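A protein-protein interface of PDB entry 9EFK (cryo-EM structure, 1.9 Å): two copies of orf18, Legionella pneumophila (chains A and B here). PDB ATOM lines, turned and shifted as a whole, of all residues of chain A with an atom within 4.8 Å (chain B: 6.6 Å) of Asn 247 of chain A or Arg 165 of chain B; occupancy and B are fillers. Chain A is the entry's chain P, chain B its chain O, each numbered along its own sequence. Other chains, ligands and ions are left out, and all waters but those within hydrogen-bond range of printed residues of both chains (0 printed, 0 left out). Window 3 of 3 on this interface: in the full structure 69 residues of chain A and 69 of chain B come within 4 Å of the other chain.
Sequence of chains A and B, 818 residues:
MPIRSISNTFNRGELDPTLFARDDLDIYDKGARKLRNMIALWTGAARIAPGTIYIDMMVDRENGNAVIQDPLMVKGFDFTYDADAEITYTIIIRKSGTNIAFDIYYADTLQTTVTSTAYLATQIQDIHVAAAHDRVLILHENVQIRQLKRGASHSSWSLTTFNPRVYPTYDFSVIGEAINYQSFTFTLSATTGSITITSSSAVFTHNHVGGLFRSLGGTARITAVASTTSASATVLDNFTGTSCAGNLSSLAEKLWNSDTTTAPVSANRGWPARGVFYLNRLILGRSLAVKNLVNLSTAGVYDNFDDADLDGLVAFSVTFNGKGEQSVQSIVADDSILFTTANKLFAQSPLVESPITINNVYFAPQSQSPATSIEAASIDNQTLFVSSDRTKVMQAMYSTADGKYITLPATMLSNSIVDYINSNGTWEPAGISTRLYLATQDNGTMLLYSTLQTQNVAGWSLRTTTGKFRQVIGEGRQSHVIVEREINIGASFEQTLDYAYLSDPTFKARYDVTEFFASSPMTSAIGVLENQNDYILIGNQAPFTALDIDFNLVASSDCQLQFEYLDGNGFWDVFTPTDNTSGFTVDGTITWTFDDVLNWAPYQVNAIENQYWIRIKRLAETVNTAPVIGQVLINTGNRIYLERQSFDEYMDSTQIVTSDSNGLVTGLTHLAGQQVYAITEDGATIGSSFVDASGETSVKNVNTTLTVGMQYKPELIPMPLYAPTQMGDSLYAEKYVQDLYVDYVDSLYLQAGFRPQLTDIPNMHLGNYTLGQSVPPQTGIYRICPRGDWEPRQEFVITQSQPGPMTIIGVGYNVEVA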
ATOM      1  N   ASP A 171       8.321 -19.858 -10.822  1.00  0.00           N
ATOM      2  CA  ASP A 171       8.576 -18.828 -11.824  1.00  0.00           C
ATOM      3  C   ASP A 171       8.105 -19.371 -13.168  1.00  0.00           C
ATOM      4  O   ASP A 171       8.813 -20.141 -13.819  1.00  0.00           O
ATOM      5  CB  ASP A 171      10.054 -18.458 -11.849  1.00  0.00           C
ATOM      6  CG  ASP A 171      10.374 -17.412 -12.887  1.00  0.00           C
ATOM      7  OD1 ASP A 171       9.439 -16.831 -13.467  1.00  0.00           O
ATOM      8  OD2 ASP A 171      11.570 -17.167 -13.124  1.00  0.00           O
ATOM      9  N   SER A 173       7.722 -17.883 -16.010  1.00  0.00           N
ATOM     10  CA  SER A 173       8.419 -17.402 -17.196  1.00  0.00           C
ATOM     11  C   SER A 173       9.515 -18.358 -17.641  1.00  0.00           C
ATOM     12  O   SER A 173       9.952 -18.291 -18.793  1.00  0.00           O
ATOM     13  CB  SER A 173       9.016 -16.022 -16.939  1.00  0.00           C
ATOM     14  OG  SER A 173      10.110 -16.112 -16.053  1.00  0.00           O
ATOM     15  N   VAL A 174       9.969 -19.241 -16.752  1.00  0.00           N
ATOM     16  CA  VAL A 174      10.988 -20.217 -17.113  1.00  0.00           C
ATOM     17  C   VAL A 174      10.456 -21.192 -18.154  1.00  0.00           C
ATOM     18  O   VAL A 174      11.199 -21.633 -19.039  1.00  0.00           O
ATOM     19  CB  VAL A 174      11.489 -20.938 -15.851  1.00  0.00           C
ATOM     20  CG1 VAL A 174      12.603 -21.871 -16.194  1.00  0.00           C
ATOM     21  CG2 VAL A 174      11.973 -19.932 -14.836  1.00  0.00           C
ATOM     22  N   TYR A 181      10.979 -11.275 -18.011  1.00  0.00           N
ATOM     23  CA  TYR A 181      11.521 -10.077 -17.383  1.00  0.00           C
ATOM     24  C   TYR A 181      13.040 -10.002 -17.477  1.00  0.00           C
ATOM     25  O   TYR A 181      13.664  -9.255 -16.718  1.00  0.00           O
ATOM     26  CB  TYR A 181      11.079 -10.003 -15.920  1.00  0.00           C
ATOM     27  CG  TYR A 181      11.441 -11.223 -15.104  1.00  0.00           C
ATOM     28  CD1 TYR A 181      12.700 -11.359 -14.546  1.00  0.00           C
ATOM     29  CD2 TYR A 181      10.520 -12.233 -14.890  1.00  0.00           C
ATOM     30  CE1 TYR A 181      13.033 -12.464 -13.807  1.00  0.00           C
ATOM     31  CE2 TYR A 181      10.846 -13.344 -14.149  1.00  0.00           C
ATOM     32  CZ  TYR A 181      12.104 -13.453 -13.611  1.00  0.00           C
ATOM     33  OH  TYR A 181      12.440 -14.556 -12.870  1.00  0.00           O
ATOM     34  N   GLN A 182      13.653 -10.757 -18.391  1.00  0.00           N
ATOM     35  CA  GLN A 182      15.109 -10.813 -18.440  1.00  0.00           C
ATOM     36  C   GLN A 182      15.732  -9.488 -18.856  1.00  0.00           C
ATOM     37  O   GLN A 182      16.903  -9.249 -18.546  1.00  0.00           O
ATOM     38  CB  GLN A 182      15.568 -11.924 -19.386  1.00  0.00           C
ATOM     39  CG  GLN A 182      15.497 -11.577 -20.858  1.00  0.00           C
ATOM     40  CD  GLN A 182      15.902 -12.734 -21.746  1.00  0.00           C
ATOM     41  OE1 GLN A 182      15.296 -13.801 -21.705  1.00  0.00           O
ATOM     42  NE2 GLN A 182      16.937 -12.531 -22.549  1.00  0.00           N
ATOM     43  N   ALA A 245      19.221  -6.299 -11.827  1.00  0.00           N
ATOM     44  CA  ALA A 245      19.046  -6.596 -13.239  1.00  0.00           C
ATOM     45  C   ALA A 245      18.042  -7.725 -13.414  1.00  0.00           C
ATOM     46  O   ALA A 245      18.022  -8.684 -12.641  1.00  0.00           O
ATOM     47  CB  ALA A 245      20.381  -6.974 -13.876  1.00  0.00           C
ATOM     48  N   GLY A 246      17.200  -7.605 -14.440  1.00  0.00           N
ATOM     49  CA  GLY A 246      16.153  -8.591 -14.640  1.00  0.00           C
ATOM     50  C   GLY A 246      16.690  -9.982 -14.910  1.00  0.00           C
ATOM     51  O   GLY A 246      16.122 -10.976 -14.455  1.00  0.00           O
ATOM     52  N   ASN A 247      17.791 -10.074 -15.653  1.00  0.00           N
ATOM     53  CA  ASN A 247      18.347 -11.373 -16.002  1.00  0.00           C
ATOM     54  C   ASN A 247      19.079 -12.040 -14.848  1.00  0.00           C
ATOM     55  O   ASN A 247      19.347 -13.243 -14.924  1.00  0.00           O
ATOM     56  CB  ASN A 247      19.287 -11.244 -17.206  1.00  0.00           C
ATOM     57  CG  ASN A 247      20.553 -10.487 -16.883  1.00  0.00           C
ATOM     58  OD1 ASN A 247      20.556  -9.574 -16.064  1.00  0.00           O
ATOM     59  ND2 ASN A 247      21.642 -10.863 -17.535  1.00  0.00           N
ATOM     60  N   LEU A 248      19.407 -11.304 -13.791  1.00  0.00           N
ATOM     61  CA  LEU A 248      20.055 -11.870 -12.618  1.00  0.00           C
ATOM     62  C   LEU A 248      19.092 -12.071 -11.454  1.00  0.00           C
ATOM     63  O   LEU A 248      19.525 -12.468 -10.370  1.00  0.00           O
ATOM     64  CB  LEU A 248      21.219 -10.984 -12.181  1.00  0.00           C
ATOM     65  CG  LEU A 248      22.323 -10.744 -13.208  1.00  0.00           C
ATOM     66  CD1 LEU A 248      23.387  -9.840 -12.626  1.00  0.00           C
ATOM     67  CD2 LEU A 248      22.928 -12.056 -13.664  1.00  0.00           C
ATOM     68  N   SER A 249      17.806 -11.820 -11.655  1.00  0.00           N
ATOM     69  CA  SER A 249      16.804 -11.901 -10.603  1.00  0.00           C
ATOM     70  C   SER A 249      15.930 -13.133 -10.794  1.00  0.00           C
ATOM     71  O   SER A 249      16.069 -13.889 -11.757  1.00  0.00           O
ATOM     72  CB  SER A 249      15.952 -10.633 -10.576  1.00  0.00           C
ATOM     73  OG  SER A 249      16.751  -9.494 -10.334  1.00  0.00           O
ATOM     74  N   ASN B 163      16.584 -16.846 -26.347  1.00  0.00           N
ATOM     75  CA  ASN B 163      17.610 -15.919 -25.884  1.00  0.00           C
ATOM     76  C   ASN B 163      17.982 -16.222 -24.441  1.00  0.00           C
ATOM     77  O   ASN B 163      17.144 -16.050 -23.544  1.00  0.00           O
ATOM     78  CB  ASN B 163      17.128 -14.476 -26.014  1.00  0.00           C
ATOM     79  CG  ASN B 163      16.774 -14.111 -27.435  1.00  0.00           C
ATOM     80  OD1 ASN B 163      17.646 -13.806 -28.245  1.00  0.00           O
ATOM     81  ND2 ASN B 163      15.486 -14.135 -27.747  1.00  0.00           N
ATOM     82  N   PRO B 164      19.203 -16.674 -24.168  1.00  0.00           N
ATOM     83  CA  PRO B 164      19.595 -16.947 -22.782  1.00  0.00           C
ATOM     84  C   PRO B 164      19.612 -15.681 -21.942  1.00  0.00           C
ATOM     85  O   PRO B 164      19.925 -14.592 -22.426  1.00  0.00           O
ATOM     86  CB  PRO B 164      21.003 -17.537 -22.920  1.00  0.00           C
ATOM     87  CG  PRO B 164      21.104 -17.974 -24.334  1.00  0.00           C
ATOM     88  CD  PRO B 164      20.266 -17.025 -25.119  1.00  0.00           C
ATOM     89  N   ARG B 165      19.273 -15.837 -20.660  1.00  0.00           N
ATOM     90  CA  ARG B 165      19.427 -14.731 -19.722  1.00  0.00           C
ATOM     91  C   ARG B 165      20.886 -14.314 -19.619  1.00  0.00           C
ATOM     92  O   ARG B 165      21.216 -13.128 -19.716  1.00  0.00           O
ATOM     93  CB  ARG B 165      18.887 -15.122 -18.348  1.00  0.00           C
ATOM     94  CG  ARG B 165      17.436 -15.554 -18.334  1.00  0.00           C
ATOM     95  CD  ARG B 165      16.948 -15.743 -16.910  1.00  0.00           C
ATOM     96  NE  ARG B 165      15.561 -16.187 -16.854  1.00  0.00           N
ATOM     97  CZ  ARG B 165      14.831 -16.225 -15.748  1.00  0.00           C
ATOM     98  NH1 ARG B 165      15.319 -15.829 -14.584  1.00  0.00           N
ATOM     99  NH2 ARG B 165      13.581 -16.671 -15.811  1.00  0.00           N
ATOM    100  N   VAL B 166      21.774 -15.283 -19.420  1.00  0.00           N
ATOM    101  CA  VAL B 166      23.215 -15.068 -19.418  1.00  0.00           C
ATOM    102  C   VAL B 166      23.849 -16.143 -20.285  1.00  0.00           C
ATOM    103  O   VAL B 166      23.506 -17.324 -20.168  1.00  0.00           O
ATOM    104  CB  VAL B 166      23.807 -15.109 -17.992  1.00  0.00           C
ATOM    105  CG1 VAL B 166      25.278 -14.748 -18.023  1.00  0.00           C
ATOM    106  CG2 VAL B 166      23.047 -14.189 -17.059  1.00  0.00           C
ATOM    107  N   TYR B 167      24.759 -15.740 -21.156  1.00  0.00           N
ATOM    108  CA  TYR B 167      25.427 -16.695 -22.024  1.00  0.00           C
ATOM    109  C   TYR B 167      26.494 -17.480 -21.266  1.00  0.00           C
ATOM    110  O   TYR B 167      27.098 -16.967 -20.323  1.00  0.00           O
ATOM    111  CB  TYR B 167      26.075 -15.982 -23.202  1.00  0.00           C
ATOM    112  CG  TYR B 167      25.123 -15.620 -24.308  1.00  0.00           C
ATOM    113  CD1 TYR B 167      24.155 -14.647 -24.125  1.00  0.00           C
ATOM    114  CD2 TYR B 167      25.202 -16.239 -25.542  1.00  0.00           C
ATOM    115  CE1 TYR B 167      23.288 -14.312 -25.133  1.00  0.00           C
ATOM    116  CE2 TYR B 167      24.340 -15.910 -26.557  1.00  0.00           C
ATOM    117  CZ  TYR B 167      23.383 -14.945 -26.348  1.00  0.00           C
ATOM    118  OH  TYR B 167      22.518 -14.611 -27.359  1.00  0.00           O
ATOM    119  N   VAL B 301      16.234 -22.987 -13.910  1.00  0.00           N
ATOM    120  CA  VAL B 301      16.079 -21.897 -14.869  1.00  0.00           C
ATOM    121  C   VAL B 301      16.667 -22.396 -16.182  1.00  0.00           C
ATOM    122  O   VAL B 301      17.881 -22.323 -16.392  1.00  0.00           O
ATOM    123  CB  VAL B 301      16.764 -20.607 -14.412  1.00  0.00           C
ATOM    124  CG1 VAL B 301      16.307 -19.443 -15.263  1.00  0.00           C
ATOM    125  CG2 VAL B 301      16.477 -20.346 -12.951  1.00  0.00           C
ATOM    126  N   ASP B 303      16.727 -21.396 -19.212  1.00  0.00           N
ATOM    127  CA  ASP B 303      17.287 -20.469 -20.183  1.00  0.00           C
ATOM    128  C   ASP B 303      18.425 -19.628 -19.621  1.00  0.00           C
ATOM    129  O   ASP B 303      18.811 -18.641 -20.247  1.00  0.00           O
ATOM    130  CB  ASP B 303      16.189 -19.563 -20.744  1.00  0.00           C
ATOM    131  CG  ASP B 303      15.564 -18.666 -19.691  1.00  0.00           C
ATOM    132  OD1 ASP B 303      15.516 -19.054 -18.508  1.00  0.00           O
ATOM    133  OD2 ASP B 303      15.106 -17.564 -20.054  1.00  0.00           O
ATOM    134  N   ASN B 304      18.969 -19.986 -18.465  1.00  0.00           N
ATOM    135  CA  ASN B 304      20.071 -19.254 -17.858  1.00  0.00           C
ATOM    136  C   ASN B 304      21.305 -20.140 -17.817  1.00  0.00           C
ATOM    137  O   ASN B 304      21.258 -21.248 -17.278  1.00  0.00           O
ATOM    138  CB  ASN B 304      19.710 -18.788 -16.448  1.00  0.00           C
ATOM    139  CG  ASN B 304      20.808 -17.978 -15.809  1.00  0.00           C
ATOM    140  OD1 ASN B 304      21.687 -17.461 -16.491  1.00  0.00           O
ATOM    141  ND2 ASN B 304      20.767 -17.860 -14.493  1.00  0.00           N
ATOM    142  N   PHE B 305      22.408 -19.644 -18.373  1.00  0.00           N
ATOM    143  CA  PHE B 305      23.665 -20.378 -18.409  1.00  0.00           C
ATOM    144  C   PHE B 305      24.788 -19.579 -17.762  1.00  0.00           C
ATOM    145  O   PHE B 305      25.941 -19.660 -18.181  1.00  0.00           O
ATOM    146  CB  PHE B 305      24.025 -20.761 -19.843  1.00  0.00           C
ATOM    147  CG  PHE B 305      23.095 -21.765 -20.443  1.00  0.00           C
ATOM    148  CD1 PHE B 305      21.916 -21.365 -21.040  1.00  0.00           C
ATOM    149  CD2 PHE B 305      23.387 -23.113 -20.390  1.00  0.00           C
ATOM    150  CE1 PHE B 305      21.054 -22.289 -21.579  1.00  0.00           C
ATOM    151  CE2 PHE B 305      22.527 -24.040 -20.928  1.00  0.00           C
ATOM    152  CZ  PHE B 305      21.361 -23.627 -21.525  1.00  0.00           C
ATOM    153  N   ASP B 306      24.453 -18.809 -16.732  1.00  0.00           N
ATOM    154  CA  ASP B 306      25.431 -17.992 -16.025  1.00  0.00           C
ATOM    155  C   ASP B 306      26.391 -18.884 -15.251  1.00  0.00           C
ATOM    156  O   ASP B 306      25.974 -19.629 -14.359  1.00  0.00           O
ATOM    157  CB  ASP B 306      24.713 -17.032 -15.080  1.00  0.00           C
ATOM    158  CG  ASP B 306      25.658 -16.071 -14.387  1.00  0.00           C
ATOM    159  OD1 ASP B 306      26.860 -16.061 -14.716  1.00  0.00           O
ATOM    160  OD2 ASP B 306      25.193 -15.314 -13.511  1.00  0.00           O
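The backbone carbonyl oxygen of Asn 163 of chain B lies close to the side-chain amide oxygen of Gln 182 of chain A (3.4 Å). The side-chain carboxylate (OD2) of Asp 171 of chain A is in salt-bridge range of the guanidinium group (NH2) of Arg 165 of chain B, 3.4 Å away. O of Arg 165 of chain B is in hydrogen-bond range of ND2 of Asn 247 of chain A (3.2 Å).
The guanidinium group of Arg 165 of chain B is in salt-bridge range of the side-chain carboxylate of Asp 303 of chain B, at 3.3 Å. O of Val 166 of chain B sits at hydrogen-bond distance from N of Phe 305 of chain B (3.1 Å). The side-chain hydroxyl (OG) of Ser 173 of chain A sits at hydrogen-bond distance from the side-chain carboxylate (OD1) of Asp 171 of chain A (2.8 Å). The side-chain hydroxyl of Tyr 181 of chain A lies within hydrogen-bond range of the side-chain carboxylate of Asp 171 of chain A (2.8 Å). The backbone carbonyl oxygen (O) of Gln 182 of chain A sits at hydrogen-bond distance from the backbone NH (N) of Asn 247 of chain A, at 3.1 Å. The backbone carbonyl oxygen (O) of Ala 245 of chain A is in hydrogen-bond range of the side-chain hydroxyl (OG) of Ser 249 of chain A (2.8 Å).
Among the printed residues, pairs that only touch across the chains: Ser 249 of chain A with Arg 165 of chain B (3.5 Å), Ser 173 of chain A with Arg 165 of chain B (3.5 Å), Tyr 181 of chain A with Arg 165 of chain B (3.6 Å), Gln 182 of chain A with Pro 164 of chain B (3.6 Å), Asn 247 of chain A with Val 166 of chain B (3.6 Å), Val 174 of chain A with Val 301 of chain B (3.7 Å), Val 174 of chain A with Arg 165 of chain B (3.8 Å) and Leu 248 of chain A with Asp 306 of chain B (3.97 Å).
Of the printed residues of chain B, Asp 171 of chain A touches Arg 165. Of the printed residues of chain A, Pro 164 of chain B touches Gln 182. Of chain A, only Asp 171 (3.4 Å), Ser 173 (3.5 Å), Val 174 (3.8 Å), Tyr 181 (3.6 Å), Asn 247 (3.2 Å) and Ser 249 (3.5 Å) come within 4 Å of Arg 165 of chain B. Of the printed residues of chain A, Val 301 of chain B touches Val 174 (3.7 Å). Asp 303 of chain B touches none of the printed residues of chain A.
Of the 10 printed residues of chain B, 6 touch a printed residue of chain A. Hydrophobic or aromatic side chains of chain B within 4 Å of the printed part of chain A: Val 166. Of the 10 printed residues of chain A, 8 touch a printed residue of chain B. Among the printed residues, Asp or Glu carboxylates within 4 Å of a Lys or Arg side-chain nitrogen of the other chain: Asp 171 of chain A with Arg 165 of chain B (3.4 Å).
No position is printed for both chains.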
